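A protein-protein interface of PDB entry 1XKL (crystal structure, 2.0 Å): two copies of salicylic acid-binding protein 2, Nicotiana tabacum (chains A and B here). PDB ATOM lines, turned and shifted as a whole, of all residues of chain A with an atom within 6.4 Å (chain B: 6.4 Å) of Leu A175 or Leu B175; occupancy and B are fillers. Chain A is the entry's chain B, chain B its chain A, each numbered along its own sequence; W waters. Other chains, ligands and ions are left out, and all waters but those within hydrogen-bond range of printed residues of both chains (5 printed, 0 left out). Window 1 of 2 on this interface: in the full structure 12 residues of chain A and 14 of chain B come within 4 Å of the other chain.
The side-chain hydroxyl (OG) of Ser A174 lies within hydrogen-bond range of the backbone carbonyl oxygen (O) of Leu A171. The side-chain carboxylate (OD1) of Asp B38 sits at hydrogen-bond distance from the backbone NH (N) of Thr B44, at 2.9 Å. The backbone carbonyl oxygen of Ala A170 is in hydrogen-bond range of the side-chain hydroxyl of Ser A174 (3.3 Å). O of Gly B43 is in hydrogen-bond range of NH1 of Arg B177 (3.0 Å). The backbone carbonyl oxygen of Cys B14 is in hydrogen-bond range of the backbone NH of Arg B177 (3.1 Å). The backbone carbonyl oxygen (O) of Gly A43 is in hydrogen-bond range of the guanidinium group (NH1) of Arg A177, 2.8 Å away.
Trp A18 touches Leu B171. Ser B174 touches Trp A18 (OG to CA, 3.4 Å). CD2 of Leu B175 touches CD1 of Trp A18, at 3.9 Å. Ser B174 touches Thr A44 (O to CG2, 3.9 Å). Leu B175 touches Thr A44. Thr A44 touches Arg B177. OG of Ser A174 touches CA of Trp B18, at 3.4 Å. Thr B44 touches Ser A174 (CG2 to O, 3.9 Å). Trp B18 touches Leu A175 (CB to CD2, 3.9 Å). CD1 of Leu B175 touches CD1 of Leu A175, at 3.5 Å.
His A15 touches none of the printed residues of chain B. Printed residues of chain B within 4 Å of Ser A174: Trp B18 and Thr B44. Printed residues of chain B within 4 Å of Leu A175: Trp B18, Thr B44 and Leu B175. His B15 touches none of the printed residues of chain A. Of chain A, only Trp A18, Thr A44 and Leu A175 come within 4 Å of Leu B175. Of the printed residues of chain A, Arg B177 touches Thr A44. The nearest printed residue of chain B that does not touch Trp A18 is Ala B170 (5.9 Å).
Of the 15 printed residues of chain B, 6 touch a printed residue of chain A. Printed residues of chain B that touch a printed residue of chain A: Trp B18, Thr B44, Leu B171, Ser B174, Leu B175 and Arg B177. Hydrophobic or aromatic side chains of chain B that line the printed part of chain A: Trp B18, Leu B171 and Leu B175. Printed residues of chain A that touch a printed residue of chain B: Trp A18, Thr A44, Leu A171, Ser A174, Leu A175 and Arg A177. Hydrophobic or aromatic side chains of chain A within 4 Å of the printed part of chain B: Trp A18, Leu A171 and Leu A175. Among the printed residues, 13 pairs touch across the chains. Among the printed residues, no Asp or Glu carboxylate lies within 4 Å of a Lys or Arg side-chain nitrogen of the other chain.
Trp A18 touches Leu B171, and with the chains exchanged Leu A171 touches Trp B18. Trp A18 touches Ser B174, and with the chains exchanged Ser A174 touches Trp B18. Trp A18 touches Leu B175, and with the chains exchanged Leu A175 touches Trp B18. Thr A44 touches Arg B177, and with the chains exchanged Arg A177 touches Thr B44. Positions printed for both chains: 14, 15, 16, 18, 38, 43, 44, 170, 171, 172, 173, 174, 175, 176 and 177. Of the 13 pairs that touch across the chains among the printed residues, 13 have their exchanged pair printed and touching as well.
Water W2 bridges the backbone carbonyl oxygen (O) of Ser B174 (2.6 Å) and the side-chain carboxylate (OD1) of Asp A38 (2.7 Å). Water W5 lies within hydrogen-bond range of O of Val B176, OG1 of Thr A44 and O of Ser B174. Water W4 lies within hydrogen-bond range of OD2 of Asp A38 (2.7 Å), N of Trp A18 (3.0 Å) and O of Ser B174 (3.1 Å). Water W1 lies within hydrogen-bond range of the side-chain carboxylate (OD2) of Asp B38, the backbone NH (N) of Trp B18 and the backbone carbonyl oxygen (O) of Ser A174. Water W3 lies within hydrogen-bond range of the backbone carbonyl oxygen of Ser A174 (2.9 Å) and the side-chain carboxylate of Asp B38 (2.9 Å).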
ATOM      1  N   CYS A  14      14.036 -21.962 -18.496  1.00  0.00           N
ATOM      2  CA  CYS A  14      14.120 -22.549 -19.824  1.00  0.00           C
ATOM      3  C   CYS A  14      14.716 -21.609 -20.862  1.00  0.00           C
ATOM      4  O   CYS A  14      14.740 -21.928 -22.048  1.00  0.00           O
ATOM      5  CB  CYS A  14      12.738 -23.027 -20.276  1.00  0.00           C
ATOM      6  SG  CYS A  14      12.038 -24.352 -19.258  1.00  0.00           S
ATOM      7  N   HIS A  15      15.193 -20.449 -20.427  1.00  0.00           N
ATOM      8  CA  HIS A  15      15.791 -19.504 -21.359  1.00  0.00           C
ATOM      9  C   HIS A  15      17.274 -19.302 -21.093  1.00  0.00           C
ATOM     10  O   HIS A  15      17.909 -20.109 -20.412  1.00  0.00           O
ATOM     11  CB  HIS A  15      15.044 -18.169 -21.312  1.00  0.00           C
ATOM     12  CG  HIS A  15      13.704 -18.222 -21.971  1.00  0.00           C
ATOM     13  ND1 HIS A  15      12.692 -19.050 -21.532  1.00  0.00           N
ATOM     14  CD2 HIS A  15      13.228 -17.606 -23.079  1.00  0.00           C
ATOM     15  CE1 HIS A  15      11.654 -18.943 -22.340  1.00  0.00           C
ATOM     16  NE2 HIS A  15      11.954 -18.072 -23.288  1.00  0.00           N
ATOM     17  N   GLY A  16      17.824 -18.231 -21.651  1.00  0.00           N
ATOM     18  CA  GLY A  16      19.233 -17.951 -21.468  1.00  0.00           C
ATOM     19  C   GLY A  16      19.544 -16.506 -21.778  1.00  0.00           C
ATOM     20  O   GLY A  16      18.643 -15.719 -22.067  1.00  0.00           O
ATOM     21  N   TRP A  18      20.645 -15.245 -24.312  1.00  0.00           N
ATOM     22  CA  TRP A  18      20.231 -14.900 -25.673  1.00  0.00           C
ATOM     23  C   TRP A  18      18.891 -14.180 -25.699  1.00  0.00           C
ATOM     24  O   TRP A  18      18.627 -13.390 -26.605  1.00  0.00           O
ATOM     25  CB  TRP A  18      20.120 -16.155 -26.550  1.00  0.00           C
ATOM     26  CG  TRP A  18      19.183 -17.199 -26.008  1.00  0.00           C
ATOM     27  CD1 TRP A  18      19.504 -18.240 -25.189  1.00  0.00           C
ATOM     28  CD2 TRP A  18      17.762 -17.275 -26.212  1.00  0.00           C
ATOM     29  NE1 TRP A  18      18.378 -18.961 -24.866  1.00  0.00           N
ATOM     30  CE2 TRP A  18      17.294 -18.391 -25.480  1.00  0.00           C
ATOM     31  CE3 TRP A  18      16.840 -16.508 -26.939  1.00  0.00           C
ATOM     32  CZ2 TRP A  18      15.940 -18.760 -25.453  1.00  0.00           C
ATOM     33  CZ3 TRP A  18      15.490 -16.877 -26.911  1.00  0.00           C
ATOM     34  CH2 TRP A  18      15.059 -17.992 -26.172  1.00  0.00           C
ATOM     35  N   ASP A  38      24.450 -16.388 -18.776  1.00  0.00           N
ATOM     36  CA  ASP A  38      23.729 -17.650 -18.868  1.00  0.00           C
ATOM     37  C   ASP A  38      23.745 -18.221 -17.449  1.00  0.00           C
ATOM     38  O   ASP A  38      24.809 -18.290 -16.829  1.00  0.00           O
ATOM     39  CB  ASP A  38      24.465 -18.647 -19.773  1.00  0.00           C
ATOM     40  CG  ASP A  38      24.059 -18.552 -21.230  1.00  0.00           C
ATOM     41  OD1 ASP A  38      24.685 -19.253 -22.060  1.00  0.00           O
ATOM     42  OD2 ASP A  38      23.115 -17.797 -21.548  1.00  0.00           O
ATOM     43  N   GLY A  43      21.160 -21.685 -21.792  1.00  0.00           N
ATOM     44  CA  GLY A  43      21.887 -21.145 -22.932  1.00  0.00           C
ATOM     45  C   GLY A  43      22.979 -22.097 -23.379  1.00  0.00           C
ATOM     46  O   GLY A  43      22.708 -23.259 -23.670  1.00  0.00           O
ATOM     47  N   THR A  44      24.218 -21.626 -23.431  1.00  0.00           N
ATOM     48  CA  THR A  44      25.292 -22.505 -23.858  1.00  0.00           C
ATOM     49  C   THR A  44      26.043 -23.132 -22.686  1.00  0.00           C
ATOM     50  O   THR A  44      27.091 -23.734 -22.885  1.00  0.00           O
ATOM     51  CB  THR A  44      26.298 -21.783 -24.779  1.00  0.00           C
ATOM     52  OG1 THR A  44      26.926 -20.703 -24.078  1.00  0.00           O
ATOM     53  CG2 THR A  44      25.591 -21.245 -26.012  1.00  0.00           C
ATOM     54  N   ALA A 170      10.504 -19.181 -33.227  1.00  0.00           N
ATOM     55  CA  ALA A 170      11.401 -20.162 -33.835  1.00  0.00           C
ATOM     56  C   ALA A 170      12.722 -20.151 -33.070  1.00  0.00           C
ATOM     57  O   ALA A 170      13.327 -21.195 -32.836  1.00  0.00           O
ATOM     58  CB  ALA A 170      11.639 -19.814 -35.299  1.00  0.00           C
ATOM     59  N   LEU A 171      13.170 -18.964 -32.684  1.00  0.00           N
ATOM     60  CA  LEU A 171      14.408 -18.851 -31.934  1.00  0.00           C
ATOM     61  C   LEU A 171      14.248 -19.585 -30.604  1.00  0.00           C
ATOM     62  O   LEU A 171      15.097 -20.384 -30.219  1.00  0.00           O
ATOM     63  CB  LEU A 171      14.747 -17.385 -31.686  1.00  0.00           C
ATOM     64  CG  LEU A 171      16.075 -17.091 -30.982  1.00  0.00           C
ATOM     65  CD1 LEU A 171      17.248 -17.610 -31.799  1.00  0.00           C
ATOM     66  CD2 LEU A 171      16.198 -15.586 -30.769  1.00  0.00           C
ATOM     67  N   ALA A 172      13.149 -19.330 -29.905  1.00  0.00           N
ATOM     68  CA  ALA A 172      12.925 -19.986 -28.627  1.00  0.00           C
ATOM     69  C   ALA A 172      12.845 -21.502 -28.755  1.00  0.00           C
ATOM     70  O   ALA A 172      13.455 -22.231 -27.968  1.00  0.00           O
ATOM     71  CB  ALA A 172      11.662 -19.447 -27.972  1.00  0.00           C
ATOM     72  N   SER A 173      12.098 -21.986 -29.743  1.00  0.00           N
ATOM     73  CA  SER A 173      11.951 -23.429 -29.937  1.00  0.00           C
ATOM     74  C   SER A 173      13.274 -24.153 -30.179  1.00  0.00           C
ATOM     75  O   SER A 173      13.405 -25.337 -29.871  1.00  0.00           O
ATOM     76  CB  SER A 173      10.994 -23.708 -31.097  1.00  0.00           C
ATOM     77  OG  SER A 173       9.701 -23.211 -30.801  1.00  0.00           O
ATOM     78  N   SER A 174      14.260 -23.449 -30.717  1.00  0.00           N
ATOM     79  CA  SER A 174      15.549 -24.086 -30.977  1.00  0.00           C
ATOM     80  C   SER A 174      16.530 -23.898 -29.825  1.00  0.00           C
ATOM     81  O   SER A 174      17.577 -24.542 -29.791  1.00  0.00           O
ATOM     82  CB  SER A 174      16.168 -23.513 -32.244  1.00  0.00           C
ATOM     83  OG  SER A 174      16.437 -22.131 -32.079  1.00  0.00           O
ATOM     84  N   LEU A 175      16.190 -23.024 -28.883  1.00  0.00           N
ATOM     85  CA  LEU A 175      17.080 -22.739 -27.764  1.00  0.00           C
ATOM     86  C   LEU A 175      16.627 -23.117 -26.352  1.00  0.00           C
ATOM     87  O   LEU A 175      17.471 -23.267 -25.460  1.00  0.00           O
ATOM     88  CB  LEU A 175      17.453 -21.257 -27.789  1.00  0.00           C
ATOM     89  CG  LEU A 175      18.364 -20.819 -28.935  1.00  0.00           C
ATOM     90  CD1 LEU A 175      18.522 -19.299 -28.933  1.00  0.00           C
ATOM     91  CD2 LEU A 175      19.721 -21.497 -28.775  1.00  0.00           C
ATOM     92  N   VAL A 176      15.322 -23.271 -26.130  1.00  0.00           N
ATOM     93  CA  VAL A 176      14.832 -23.611 -24.785  1.00  0.00           C
ATOM     94  C   VAL A 176      15.428 -24.908 -24.227  1.00  0.00           C
ATOM     95  O   VAL A 176      15.645 -25.872 -24.963  1.00  0.00           O
ATOM     96  CB  VAL A 176      13.271 -23.740 -24.737  1.00  0.00           C
ATOM     97  CG1 VAL A 176      12.622 -22.371 -24.919  1.00  0.00           C
ATOM     98  CG2 VAL A 176      12.775 -24.718 -25.808  1.00  0.00           C
ATOM     99  N   ARG A 177      15.696 -24.925 -22.924  1.00  0.00           N
ATOM    100  CA  ARG A 177      16.244 -26.111 -22.269  1.00  0.00           C
ATOM    101  C   ARG A 177      15.501 -26.377 -20.964  1.00  0.00           C
ATOM    102  O   ARG A 177      14.924 -25.462 -20.387  1.00  0.00           O
ATOM    103  CB  ARG A 177      17.735 -25.910 -21.962  1.00  0.00           C
ATOM    104  CG  ARG A 177      18.559 -25.607 -23.190  1.00  0.00           C
ATOM    105  CD  ARG A 177      19.980 -25.329 -22.814  1.00  0.00           C
ATOM    106  NE  ARG A 177      20.547 -26.395 -21.987  1.00  0.00           N
ATOM    107  CZ  ARG A 177      21.762 -26.328 -21.457  1.00  0.00           C
ATOM    108  NH1 ARG A 177      22.513 -25.255 -21.678  1.00  0.00           N
ATOM    109  NH2 ARG A 177      22.222 -27.310 -20.706  1.00  0.00           N
ATOM    110  N   CYS B  14      30.705 -23.318 -34.839  1.00  0.00           N
ATOM    111  CA  CYS B  14      30.468 -22.441 -33.702  1.00  0.00           C
ATOM    112  C   CYS B  14      29.025 -21.946 -33.629  1.00  0.00           C
ATOM    113  O   CYS B  14      28.691 -21.176 -32.731  1.00  0.00           O
ATOM    114  CB  CYS B  14      31.422 -21.242 -33.742  1.00  0.00           C
ATOM    115  SG  CYS B  14      33.199 -21.645 -33.676  1.00  0.00           S
ATOM    116  N   HIS B  15      28.179 -22.374 -34.565  1.00  0.00           N
ATOM    117  CA  HIS B  15      26.775 -21.953 -34.565  1.00  0.00           C
ATOM    118  C   HIS B  15      25.828 -23.110 -34.268  1.00  0.00           C
ATOM    119  O   HIS B  15      26.266 -24.172 -33.826  1.00  0.00           O
ATOM    120  CB  HIS B  15      26.413 -21.293 -35.903  1.00  0.00           C
ATOM    121  CG  HIS B  15      27.027 -19.939 -36.087  1.00  0.00           C
ATOM    122  ND1 HIS B  15      28.390 -19.743 -36.167  1.00  0.00           N
ATOM    123  CD2 HIS B  15      26.466 -18.706 -36.148  1.00  0.00           C
ATOM    124  CE1 HIS B  15      28.643 -18.450 -36.264  1.00  0.00           C
ATOM    125  NE2 HIS B  15      27.492 -17.798 -36.255  1.00  0.00           N
ATOM    126  N   GLY B  16      24.532 -22.901 -34.489  1.00  0.00           N
ATOM    127  CA  GLY B  16      23.550 -23.947 -34.226  1.00  0.00           C
ATOM    128  C   GLY B  16      22.238 -23.739 -34.972  1.00  0.00           C
ATOM    129  O   GLY B  16      22.111 -22.800 -35.752  1.00  0.00           O
ATOM    130  N   TRP B  18      19.705 -22.447 -34.118  1.00  0.00           N
ATOM    131  CA  TRP B  18      19.201 -21.115 -33.839  1.00  0.00           C
ATOM    132  C   TRP B  18      19.513 -20.092 -34.935  1.00  0.00           C
ATOM    133  O   TRP B  18      18.744 -19.154 -35.138  1.00  0.00           O
ATOM    134  CB  TRP B  18      19.771 -20.600 -32.523  1.00  0.00           C
ATOM    135  CG  TRP B  18      21.266 -20.517 -32.492  1.00  0.00           C
ATOM    136  CD1 TRP B  18      22.133 -21.459 -32.011  1.00  0.00           C
ATOM    137  CD2 TRP B  18      22.072 -19.408 -32.908  1.00  0.00           C
ATOM    138  NE1 TRP B  18      23.429 -21.000 -32.091  1.00  0.00           N
ATOM    139  CE2 TRP B  18      23.420 -19.744 -32.638  1.00  0.00           C
ATOM    140  CE3 TRP B  18      21.789 -18.162 -33.479  1.00  0.00           C
ATOM    141  CZ2 TRP B  18      24.480 -18.877 -32.917  1.00  0.00           C
ATOM    142  CZ3 TRP B  18      22.840 -17.297 -33.760  1.00  0.00           C
ATOM    143  CH2 TRP B  18      24.174 -17.660 -33.476  1.00  0.00           C
ATOM    144  N   ASP B  38      20.641 -29.230 -34.611  1.00  0.00           N
ATOM    145  CA  ASP B  38      21.855 -28.830 -33.928  1.00  0.00           C
ATOM    146  C   ASP B  38      22.827 -29.963 -34.196  1.00  0.00           C
ATOM    147  O   ASP B  38      22.488 -31.124 -33.974  1.00  0.00           O
ATOM    148  CB  ASP B  38      21.625 -28.747 -32.418  1.00  0.00           C
ATOM    149  CG  ASP B  38      21.164 -27.379 -31.952  1.00  0.00           C
ATOM    150  OD1 ASP B  38      20.703 -27.298 -30.792  1.00  0.00           O
ATOM    151  OD2 ASP B  38      21.269 -26.389 -32.708  1.00  0.00           O
ATOM    152  N   GLY B  43      24.749 -25.559 -30.520  1.00  0.00           N
ATOM    153  CA  GLY B  43      23.448 -25.116 -30.049  1.00  0.00           C
ATOM    154  C   GLY B  43      23.218 -25.584 -28.627  1.00  0.00           C
ATOM    155  O   GLY B  43      24.001 -25.265 -27.732  1.00  0.00           O
ATOM    156  N   THR B  44      22.163 -26.356 -28.411  1.00  0.00           N
ATOM    157  CA  THR B  44      21.870 -26.854 -27.072  1.00  0.00           C
ATOM    158  C   THR B  44      22.334 -28.292 -26.855  1.00  0.00           C
ATOM    159  O   THR B  44      22.041 -28.892 -25.818  1.00  0.00           O
ATOM    160  CB  THR B  44      20.349 -26.745 -26.747  1.00  0.00           C
ATOM    161  OG1 THR B  44      19.586 -27.503 -27.695  1.00  0.00           O
ATOM    162  CG2 THR B  44      19.906 -25.292 -26.780  1.00  0.00           C
ATOM    163  N   ALA B 170      24.654  -9.445 -31.080  1.00  0.00           N
ATOM    164  CA  ALA B 170      24.452  -9.703 -29.652  1.00  0.00           C
ATOM    165  C   ALA B 170      23.975 -11.137 -29.451  1.00  0.00           C
ATOM    166  O   ALA B 170      24.374 -11.812 -28.504  1.00  0.00           O
ATOM    167  CB  ALA B 170      23.437  -8.729 -29.084  1.00  0.00           C
ATOM    168  N   LEU B 171      23.117 -11.598 -30.355  1.00  0.00           N
ATOM    169  CA  LEU B 171      22.592 -12.947 -30.284  1.00  0.00           C
ATOM    170  C   LEU B 171      23.710 -13.961 -30.527  1.00  0.00           C
ATOM    171  O   LEU B 171      23.908 -14.888 -29.730  1.00  0.00           O
ATOM    172  CB  LEU B 171      21.475 -13.115 -31.316  1.00  0.00           C
ATOM    173  CG  LEU B 171      20.791 -14.478 -31.434  1.00  0.00           C
ATOM    174  CD1 LEU B 171      20.089 -14.834 -30.138  1.00  0.00           C
ATOM    175  CD2 LEU B 171      19.794 -14.436 -32.589  1.00  0.00           C
ATOM    176  N   ALA B 172      24.459 -13.782 -31.613  1.00  0.00           N
ATOM    177  CA  ALA B 172      25.549 -14.710 -31.918  1.00  0.00           C
ATOM    178  C   ALA B 172      26.575 -14.766 -30.789  1.00  0.00           C
ATOM    179  O   ALA B 172      27.029 -15.843 -30.411  1.00  0.00           O
ATOM    180  CB  ALA B 172      26.238 -14.312 -33.227  1.00  0.00           C
ATOM    181  N   SER B 173      26.938 -13.607 -30.249  1.00  0.00           N
ATOM    182  CA  SER B 173      27.923 -13.568 -29.186  1.00  0.00           C
ATOM    183  C   SER B 173      27.526 -14.366 -27.950  1.00  0.00           C
ATOM    184  O   SER B 173      28.382 -14.928 -27.268  1.00  0.00           O
ATOM    185  CB  SER B 173      28.227 -12.124 -28.793  1.00  0.00           C
ATOM    186  OG  SER B 173      28.928 -11.460 -29.829  1.00  0.00           O
ATOM    187  N   SER B 174      26.235 -14.433 -27.656  1.00  0.00           N
ATOM    188  CA  SER B 174      25.790 -15.174 -26.482  1.00  0.00           C
ATOM    189  C   SER B 174      25.518 -16.647 -26.769  1.00  0.00           C
ATOM    190  O   SER B 174      25.204 -17.401 -25.855  1.00  0.00           O
ATOM    191  CB  SER B 174      24.522 -14.549 -25.909  1.00  0.00           C
ATOM    192  OG  SER B 174      23.434 -14.772 -26.785  1.00  0.00           O
ATOM    193  N   LEU B 175      25.635 -17.069 -28.026  1.00  0.00           N
ATOM    194  CA  LEU B 175      25.356 -18.465 -28.352  1.00  0.00           C
ATOM    195  C   LEU B 175      26.483 -19.245 -29.011  1.00  0.00           C
ATOM    196  O   LEU B 175      26.437 -20.475 -29.046  1.00  0.00           O
ATOM    197  CB  LEU B 175      24.119 -18.553 -29.240  1.00  0.00           C
ATOM    198  CG  LEU B 175      22.793 -18.155 -28.584  1.00  0.00           C
ATOM    199  CD1 LEU B 175      21.685 -18.111 -29.637  1.00  0.00           C
ATOM    200  CD2 LEU B 175      22.459 -19.156 -27.493  1.00  0.00           C
ATOM    201  N   VAL B 176      27.484 -18.550 -29.542  1.00  0.00           N
ATOM    202  CA  VAL B 176      28.586 -19.243 -30.203  1.00  0.00           C
ATOM    203  C   VAL B 176      29.336 -20.171 -29.264  1.00  0.00           C
ATOM    204  O   VAL B 176      29.567 -19.846 -28.106  1.00  0.00           O
ATOM    205  CB  VAL B 176      29.611 -18.263 -30.831  1.00  0.00           C
ATOM    206  CG1 VAL B 176      28.986 -17.563 -32.025  1.00  0.00           C
ATOM    207  CG2 VAL B 176      30.100 -17.263 -29.802  1.00  0.00           C
ATOM    208  N   ARG B 177      29.708 -21.338 -29.773  1.00  0.00           N
ATOM    209  CA  ARG B 177      30.444 -22.303 -28.982  1.00  0.00           C
ATOM    210  C   ARG B 177      31.655 -22.778 -29.772  1.00  0.00           C
ATOM    211  O   ARG B 177      31.726 -22.598 -30.992  1.00  0.00           O
ATOM    212  CB  ARG B 177      29.548 -23.497 -28.636  1.00  0.00           C
ATOM    213  CG  ARG B 177      28.347 -23.159 -27.745  1.00  0.00           C
ATOM    214  CD  ARG B 177      27.428 -24.364 -27.609  1.00  0.00           C
ATOM    215  NE  ARG B 177      28.099 -25.476 -26.942  1.00  0.00           N
ATOM    216  CZ  ARG B 177      27.606 -26.705 -26.851  1.00  0.00           C
ATOM    217  NH1 ARG B 177      26.431 -26.995 -27.388  1.00  0.00           N
ATOM    218  NH2 ARG B 177      28.289 -27.652 -26.223  1.00  0.00           N
HETATM  219  O   HOH W   1      20.256 -23.962 -31.667  1.00  0.00           O
HETATM  220  O   HOH W   2      25.960 -17.308 -23.363  1.00  0.00           O
HETATM  221  O   HOH W   3      17.841 -27.075 -31.095  1.00  0.00           O
HETATM  222  O   HOH W   4      22.541 -17.584 -24.187  1.00  0.00           O
HETATM  223  O   HOH W   5      28.482 -18.530 -26.029  1.00  0.00           O
